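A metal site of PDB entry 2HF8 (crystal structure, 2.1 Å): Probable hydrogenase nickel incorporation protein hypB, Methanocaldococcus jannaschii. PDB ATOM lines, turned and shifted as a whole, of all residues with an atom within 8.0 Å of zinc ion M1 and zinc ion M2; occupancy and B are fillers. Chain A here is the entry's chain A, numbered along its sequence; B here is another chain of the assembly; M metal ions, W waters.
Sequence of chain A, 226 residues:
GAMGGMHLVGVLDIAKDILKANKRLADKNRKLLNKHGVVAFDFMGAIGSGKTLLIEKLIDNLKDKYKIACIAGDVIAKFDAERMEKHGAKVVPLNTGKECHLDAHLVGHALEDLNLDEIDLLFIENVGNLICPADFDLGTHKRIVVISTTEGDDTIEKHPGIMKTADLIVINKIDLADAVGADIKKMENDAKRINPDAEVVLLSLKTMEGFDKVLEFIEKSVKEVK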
ATOM      1  N   LYS A  98      11.390  28.693  -5.891  1.00  0.00           N
ATOM      2  CA  LYS A  98      10.460  27.841  -6.620  1.00  0.00           C
ATOM      3  C   LYS A  98      10.394  26.413  -6.078  1.00  0.00           C
ATOM      4  O   LYS A  98       9.564  25.612  -6.509  1.00  0.00           O
ATOM      5  CB  LYS A  98      10.774  27.846  -8.127  1.00  0.00           C
ATOM      6  CG  LYS A  98      10.346  29.119  -8.844  1.00  0.00           C
ATOM      7  CD  LYS A  98      10.412  28.952 -10.359  1.00  0.00           C
ATOM      8  CE  LYS A  98       9.751  30.120 -11.064  1.00  0.00           C
ATOM      9  NZ  LYS A  98       9.797  29.972 -12.551  1.00  0.00           N
ATOM     10  N   GLU A  99      11.273  26.101  -5.119  1.00  0.00           N
ATOM     11  CA  GLU A  99      11.329  24.777  -4.496  1.00  0.00           C
ATOM     12  C   GLU A  99      10.138  24.563  -3.556  1.00  0.00           C
ATOM     13  O   GLU A  99       9.725  25.468  -2.833  1.00  0.00           O
ATOM     14  CB  GLU A  99      12.635  24.604  -3.734  1.00  0.00           C
ATOM     15  CG  GLU A  99      13.022  23.149  -3.449  1.00  0.00           C
ATOM     16  CD  GLU A  99      14.024  22.587  -4.454  1.00  0.00           C
ATOM     17  OE1 GLU A  99      13.996  22.975  -5.651  1.00  0.00           O
ATOM     18  OE2 GLU A  99      14.850  21.743  -4.029  1.00  0.00           O
ATOM     19  N   CYS A 100       9.582  23.350  -3.570  1.00  0.00           N
ATOM     20  CA  CYS A 100       8.374  23.037  -2.810  1.00  0.00           C
ATOM     21  C   CYS A 100       8.669  22.360  -1.467  1.00  0.00           C
ATOM     22  O   CYS A 100       7.753  21.898  -0.781  1.00  0.00           O
ATOM     23  CB  CYS A 100       7.419  22.191  -3.658  1.00  0.00           C
ATOM     24  SG  CYS A 100       8.214  20.845  -4.582  1.00  0.00           S
ATOM     25  N   HIS A 101       9.939  22.323  -1.089  1.00  0.00           N
ATOM     26  CA  HIS A 101      10.391  21.675   0.146  1.00  0.00           C
ATOM     27  C   HIS A 101      11.783  22.156   0.556  1.00  0.00           C
ATOM     28  O   HIS A 101      12.534  22.672  -0.267  1.00  0.00           O
ATOM     29  CB  HIS A 101      10.419  20.144  -0.042  1.00  0.00           C
ATOM     30  CG  HIS A 101      11.422  19.692  -1.053  1.00  0.00           C
ATOM     31  ND1 HIS A 101      11.131  19.603  -2.406  1.00  0.00           N
ATOM     32  CD2 HIS A 101      12.722  19.334  -0.920  1.00  0.00           C
ATOM     33  CE1 HIS A 101      12.206  19.198  -3.051  1.00  0.00           C
ATOM     34  NE2 HIS A 101      13.188  19.032  -2.179  1.00  0.00           N
ATOM     35  N   ASN A 129       3.257  23.239   3.074  1.00  0.00           N
ATOM     36  CA  ASN A 129       3.100  22.175   2.071  1.00  0.00           C
ATOM     37  C   ASN A 129       2.844  20.862   2.809  1.00  0.00           C
ATOM     38  O   ASN A 129       3.649  20.453   3.644  1.00  0.00           O
ATOM     39  CB  ASN A 129       4.371  22.074   1.209  1.00  0.00           C
ATOM     40  CG  ASN A 129       4.195  21.187  -0.027  1.00  0.00           C
ATOM     41  OD1 ASN A 129       3.364  20.283  -0.052  1.00  0.00           O
ATOM     42  ND2 ASN A 129       5.001  21.451  -1.042  1.00  0.00           N
ATOM     43  N   ILE A 131       2.560  17.908   1.327  1.00  0.00           N
ATOM     44  CA  ILE A 131       2.927  16.815   0.438  1.00  0.00           C
ATOM     45  C   ILE A 131       4.432  16.539   0.473  1.00  0.00           C
ATOM     46  O   ILE A 131       4.866  15.567   1.096  1.00  0.00           O
ATOM     47  CB  ILE A 131       2.425  17.067  -1.016  1.00  0.00           C
ATOM     48  CG1 ILE A 131       0.893  17.207  -1.017  1.00  0.00           C
ATOM     49  CG2 ILE A 131       2.874  15.932  -1.946  1.00  0.00           C
ATOM     50  CD1 ILE A 131       0.281  17.697  -2.308  1.00  0.00           C
ATOM     51  N   CYS A 132       5.214  17.393  -0.172  1.00  0.00           N
ATOM     52  CA  CYS A 132       6.638  17.152  -0.440  1.00  0.00           C
ATOM     53  C   CYS A 132       7.529  16.964   0.804  1.00  0.00           C
ATOM     54  O   CYS A 132       8.398  16.090   0.805  1.00  0.00           O
ATOM     55  CB  CYS A 132       7.212  18.237  -1.360  1.00  0.00           C
ATOM     56  SG  CYS A 132       6.019  18.862  -2.569  1.00  0.00           S
ATOM     57  N   PRO A 133       7.345  17.797   1.860  1.00  0.00           N
ATOM     58  CA  PRO A 133       8.184  17.624   3.057  1.00  0.00           C
ATOM     59  C   PRO A 133       8.170  16.236   3.732  1.00  0.00           C
ATOM     60  O   PRO A 133       9.049  15.943   4.538  1.00  0.00           O
ATOM     61  CB  PRO A 133       7.639  18.697   4.020  1.00  0.00           C
ATOM     62  CG  PRO A 133       7.057  19.730   3.113  1.00  0.00           C
ATOM     63  CD  PRO A 133       6.433  18.943   2.003  1.00  0.00           C
ATOM     64  N   ASP A 135       8.925  13.407   2.429  1.00  0.00           N
ATOM     65  CA  ASP A 135      10.058  12.594   1.940  1.00  0.00           C
ATOM     66  C   ASP A 135      11.443  13.149   2.321  1.00  0.00           C
ATOM     67  O   ASP A 135      12.450  12.462   2.133  1.00  0.00           O
ATOM     68  CB  ASP A 135       9.996  12.443   0.424  1.00  0.00           C
ATOM     69  CG  ASP A 135       8.664  11.867  -0.061  1.00  0.00           C
ATOM     70  OD1 ASP A 135       8.175  10.878   0.530  1.00  0.00           O
ATOM     71  OD2 ASP A 135       8.127  12.412  -1.058  1.00  0.00           O
ATOM     72  N   PHE A 136      11.495  14.367   2.852  1.00  0.00           N
ATOM     73  CA  PHE A 136      12.770  15.054   3.065  1.00  0.00           C
ATOM     74  C   PHE A 136      13.141  15.322   4.531  1.00  0.00           C
ATOM     75  O   PHE A 136      12.946  16.415   5.048  1.00  0.00           O
ATOM     76  CB  PHE A 136      12.823  16.345   2.232  1.00  0.00           C
ATOM     77  CG  PHE A 136      12.898  16.104   0.760  1.00  0.00           C
ATOM     78  CD1 PHE A 136      11.738  16.057  -0.015  1.00  0.00           C
ATOM     79  CD2 PHE A 136      14.135  15.923   0.127  1.00  0.00           C
ATOM     80  CE1 PHE A 136      11.813  15.823  -1.394  1.00  0.00           C
ATOM     81  CE2 PHE A 136      14.210  15.689  -1.252  1.00  0.00           C
ATOM     82  CZ  PHE A 136      13.052  15.644  -2.013  1.00  0.00           C
ATOM     83  N   LYS B  98       2.338  11.327  -5.009  1.00  0.00           N
ATOM     84  CA  LYS B  98       3.309  12.127  -4.271  1.00  0.00           C
ATOM     85  C   LYS B  98       3.697  13.372  -5.066  1.00  0.00           C
ATOM     86  O   LYS B  98       4.491  14.193  -4.605  1.00  0.00           O
ATOM     87  CB  LYS B  98       4.537  11.298  -3.888  1.00  0.00           C
ATOM     88  CG  LYS B  98       4.351  10.491  -2.616  1.00  0.00           C
ATOM     89  CD  LYS B  98       5.640   9.828  -2.181  1.00  0.00           C
ATOM     90  CE  LYS B  98       5.517   9.199  -0.794  1.00  0.00           C
ATOM     91  NZ  LYS B  98       4.519   8.096  -0.725  1.00  0.00           N
ATOM     92  N   GLU B  99       3.124  13.490  -6.267  1.00  0.00           N
ATOM     93  CA  GLU B  99       3.291  14.674  -7.101  1.00  0.00           C
ATOM     94  C   GLU B  99       2.490  15.820  -6.504  1.00  0.00           C
ATOM     95  O   GLU B  99       1.404  15.624  -5.966  1.00  0.00           O
ATOM     96  CB  GLU B  99       2.869  14.385  -8.544  1.00  0.00           C
ATOM     97  CG  GLU B  99       3.445  15.345  -9.585  1.00  0.00           C
ATOM     98  CD  GLU B  99       4.932  15.177  -9.820  1.00  0.00           C
ATOM     99  OE1 GLU B  99       5.471  14.056  -9.622  1.00  0.00           O
ATOM    100  OE2 GLU B  99       5.589  16.173 -10.215  1.00  0.00           O
ATOM    101  N   CYS B 100       3.037  17.026  -6.618  1.00  0.00           N
ATOM    102  CA  CYS B 100       2.550  18.189  -5.873  1.00  0.00           C
ATOM    103  C   CYS B 100       1.848  19.199  -6.763  1.00  0.00           C
ATOM    104  O   CYS B 100       1.539  20.309  -6.321  1.00  0.00           O
ATOM    105  CB  CYS B 100       3.720  18.842  -5.149  1.00  0.00           C
ATOM    106  SG  CYS B 100       5.293  18.666  -6.045  1.00  0.00           S
ATOM    107  N   HIS B 101       1.586  18.809  -8.013  1.00  0.00           N
ATOM    108  CA  HIS B 101       0.952  19.677  -8.994  1.00  0.00           C
ATOM    109  C   HIS B 101       0.342  18.862 -10.131  1.00  0.00           C
ATOM    110  O   HIS B 101       0.821  17.766 -10.452  1.00  0.00           O
ATOM    111  CB  HIS B 101       1.977  20.671  -9.569  1.00  0.00           C
ATOM    112  CG  HIS B 101       3.152  20.018 -10.225  1.00  0.00           C
ATOM    113  ND1 HIS B 101       4.367  19.871  -9.598  1.00  0.00           N
ATOM    114  CD2 HIS B 101       3.296  19.464 -11.460  1.00  0.00           C
ATOM    115  CE1 HIS B 101       5.211  19.251 -10.406  1.00  0.00           C
ATOM    116  NE2 HIS B 101       4.575  18.991 -11.540  1.00  0.00           N
ATOM    117  N   LEU B 102      -0.719  19.389 -10.735  1.00  0.00           N
ATOM    118  CA  LEU B 102      -1.195  18.862 -12.007  1.00  0.00           C
ATOM    119  C   LEU B 102      -0.283  19.350 -13.133  1.00  0.00           C
ATOM    120  O   LEU B 102       0.403  20.373 -12.983  1.00  0.00           O
ATOM    121  CB  LEU B 102      -2.649  19.278 -12.272  1.00  0.00           C
ATOM    122  CG  LEU B 102      -3.758  18.651 -11.422  1.00  0.00           C
ATOM    123  CD1 LEU B 102      -5.103  19.224 -11.819  1.00  0.00           C
ATOM    124  CD2 LEU B 102      -3.781  17.130 -11.555  1.00  0.00           C
ATOM    125  N   VAL B 127      -4.078  20.802  -7.366  1.00  0.00           N
ATOM    126  CA  VAL B 127      -3.668  20.380  -6.024  1.00  0.00           C
ATOM    127  C   VAL B 127      -3.486  21.604  -5.129  1.00  0.00           C
ATOM    128  O   VAL B 127      -3.029  22.652  -5.601  1.00  0.00           O
ATOM    129  CB  VAL B 127      -2.338  19.553  -6.061  1.00  0.00           C
ATOM    130  CG1 VAL B 127      -2.078  18.876  -4.729  1.00  0.00           C
ATOM    131  CG2 VAL B 127      -2.373  18.518  -7.168  1.00  0.00           C
ATOM    132  N   ASN B 129      -1.731  23.937  -3.160  1.00  0.00           N
ATOM    133  CA  ASN B 129      -0.308  24.241  -3.263  1.00  0.00           C
ATOM    134  C   ASN B 129      -0.132  25.609  -3.897  1.00  0.00           C
ATOM    135  O   ASN B 129      -0.648  25.872  -4.979  1.00  0.00           O
ATOM    136  CB  ASN B 129       0.401  23.172  -4.116  1.00  0.00           C
ATOM    137  CG  ASN B 129       1.902  23.124  -3.893  1.00  0.00           C
ATOM    138  OD1 ASN B 129       2.561  24.157  -3.727  1.00  0.00           O
ATOM    139  ND2 ASN B 129       2.469  21.918  -3.896  1.00  0.00           N
ATOM    140  N   ILE B 131       2.935  26.952  -4.561  1.00  0.00           N
ATOM    141  CA  ILE B 131       4.277  27.045  -5.131  1.00  0.00           C
ATOM    142  C   ILE B 131       4.309  26.587  -6.593  1.00  0.00           C
ATOM    143  O   ILE B 131       4.218  27.405  -7.504  1.00  0.00           O
ATOM    144  CB  ILE B 131       5.336  26.239  -4.307  1.00  0.00           C
ATOM    145  CG1 ILE B 131       5.206  26.500  -2.803  1.00  0.00           C
ATOM    146  CG2 ILE B 131       6.758  26.524  -4.817  1.00  0.00           C
ATOM    147  CD1 ILE B 131       5.202  27.958  -2.394  1.00  0.00           C
ATOM    148  N   CYS B 132       4.438  25.280  -6.798  1.00  0.00           N
ATOM    149  CA  CYS B 132       4.760  24.733  -8.112  1.00  0.00           C
ATOM    150  C   CYS B 132       3.654  24.737  -9.179  1.00  0.00           C
ATOM    151  O   CYS B 132       3.981  24.747 -10.373  1.00  0.00           O
ATOM    152  CB  CYS B 132       5.395  23.339  -7.993  1.00  0.00           C
ATOM    153  SG  CYS B 132       4.639  22.243  -6.785  1.00  0.00           S
ATOM    154  N   PRO B 133       2.357  24.738  -8.783  1.00  0.00           N
ATOM    155  CA  PRO B 133       1.327  24.918  -9.823  1.00  0.00           C
ATOM    156  C   PRO B 133       1.491  26.171 -10.693  1.00  0.00           C
ATOM    157  O   PRO B 133       0.950  26.210 -11.802  1.00  0.00           O
ATOM    158  CB  PRO B 133       0.028  24.994  -9.005  1.00  0.00           C
ATOM    159  CG  PRO B 133       0.318  24.196  -7.791  1.00  0.00           C
ATOM    160  CD  PRO B 133       1.745  24.523  -7.460  1.00  0.00           C
ATOM    161  N   ASP B 135       4.118  26.994 -12.218  1.00  0.00           N
ATOM    162  CA  ASP B 135       5.052  26.667 -13.293  1.00  0.00           C
ATOM    163  C   ASP B 135       4.447  25.783 -14.379  1.00  0.00           C
ATOM    164  O   ASP B 135       5.059  25.602 -15.440  1.00  0.00           O
ATOM    165  CB  ASP B 135       6.300  25.988 -12.707  1.00  0.00           C
ATOM    166  CG  ASP B 135       7.205  26.950 -11.960  1.00  0.00           C
ATOM    167  OD1 ASP B 135       7.799  26.531 -10.940  1.00  0.00           O
ATOM    168  OD2 ASP B 135       7.315  28.133 -12.385  1.00  0.00           O
ATOM    169  N   PHE B 136       3.271  25.222 -14.109  1.00  0.00           N
ATOM    170  CA  PHE B 136       2.688  24.192 -14.980  1.00  0.00           C
ATOM    171  C   PHE B 136       1.328  24.560 -15.580  1.00  0.00           C
ATOM    172  O   PHE B 136       0.278  24.244 -15.018  1.00  0.00           O
ATOM    173  CB  PHE B 136       2.629  22.849 -14.241  1.00  0.00           C
ATOM    174  CG  PHE B 136       3.988  22.296 -13.877  1.00  0.00           C
ATOM    175  CD1 PHE B 136       4.608  22.665 -12.689  1.00  0.00           C
ATOM    176  CD2 PHE B 136       4.641  21.416 -14.731  1.00  0.00           C
ATOM    177  CE1 PHE B 136       5.859  22.171 -12.354  1.00  0.00           C
ATOM    178  CE2 PHE B 136       5.892  20.909 -14.403  1.00  0.00           C
ATOM    179  CZ  PHE B 136       6.511  21.289 -13.223  1.00  0.00           C
HETATM  180 ZN    ZN M   1       6.926  18.840  -4.573  1.00  0.00          ZN
HETATM  181 ZN    ZN M   2       5.153  20.106  -7.561  1.00  0.00          ZN
HETATM  182  O   HOH W   1       7.360  20.159  -7.791  1.00  0.00           O
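Within 4 Å of zinc ion M1: Cys 100 of chain A, Cys 132 of chain A and Cys 100 of chain B. Along chain A the residues within 4 Å of zinc ion M1 span positions 100 to 132. The nearest printed residue that does not touch zinc ion M1 is Cys 132 of chain B (4.7 Å).
The backbone carbonyl oxygen of Cys 100 of chain B lies within hydrogen-bond range of the side-chain amide nitrogen of Asn 129 of chain B (3.1 Å). NE2 of His 101 of chain B lies close to OE2 of Glu 99 of chain B, 3.3 Å away. The side-chain amide oxygen of Asn 129 of chain A sits at hydrogen-bond distance from the backbone NH of Cys 132 of chain A, 3.4 Å away. The side-chain sulfur of Cys 132 of chain B sits close to the side-chain amide nitrogen of Asn 129 of chain B (3.6 Å). The backbone carbonyl oxygen (O) of Cys 100 of chain A lies within hydrogen-bond range of the side-chain amide nitrogen (ND2) of Asn 129 of chain A (2.8 Å).
Three residues have an atom within 4 Å of zinc ion M2: Cys 100 of chain B, His 101 of chain B and Cys 132 of chain B. The nearest printed residue that does not touch zinc ion M2 is Cys 100 of chain A (4.3 Å).
Zinc ion M1 is bound by the side-chain sulfur of Cys 132 of chain A (2.2 Å), the side-chain sulfur of Cys 100 of chain B (2.2 Å) and the side-chain sulfur of Cys 100 of chain A (2.4 Å). Zinc ion M1 has three donor atoms within binding distance.
Zinc ion M2 is bound by the side-chain sulfur (SG) of Cys 100 of chain B (2.1 Å). A ring nitrogen (ND1) of His 101 of chain B binds zinc ion M2 (2.2 Å). Water W1 is bound to zinc ion M2. SG of Cys 132 of chain B binds zinc ion M2 (2.3 Å).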
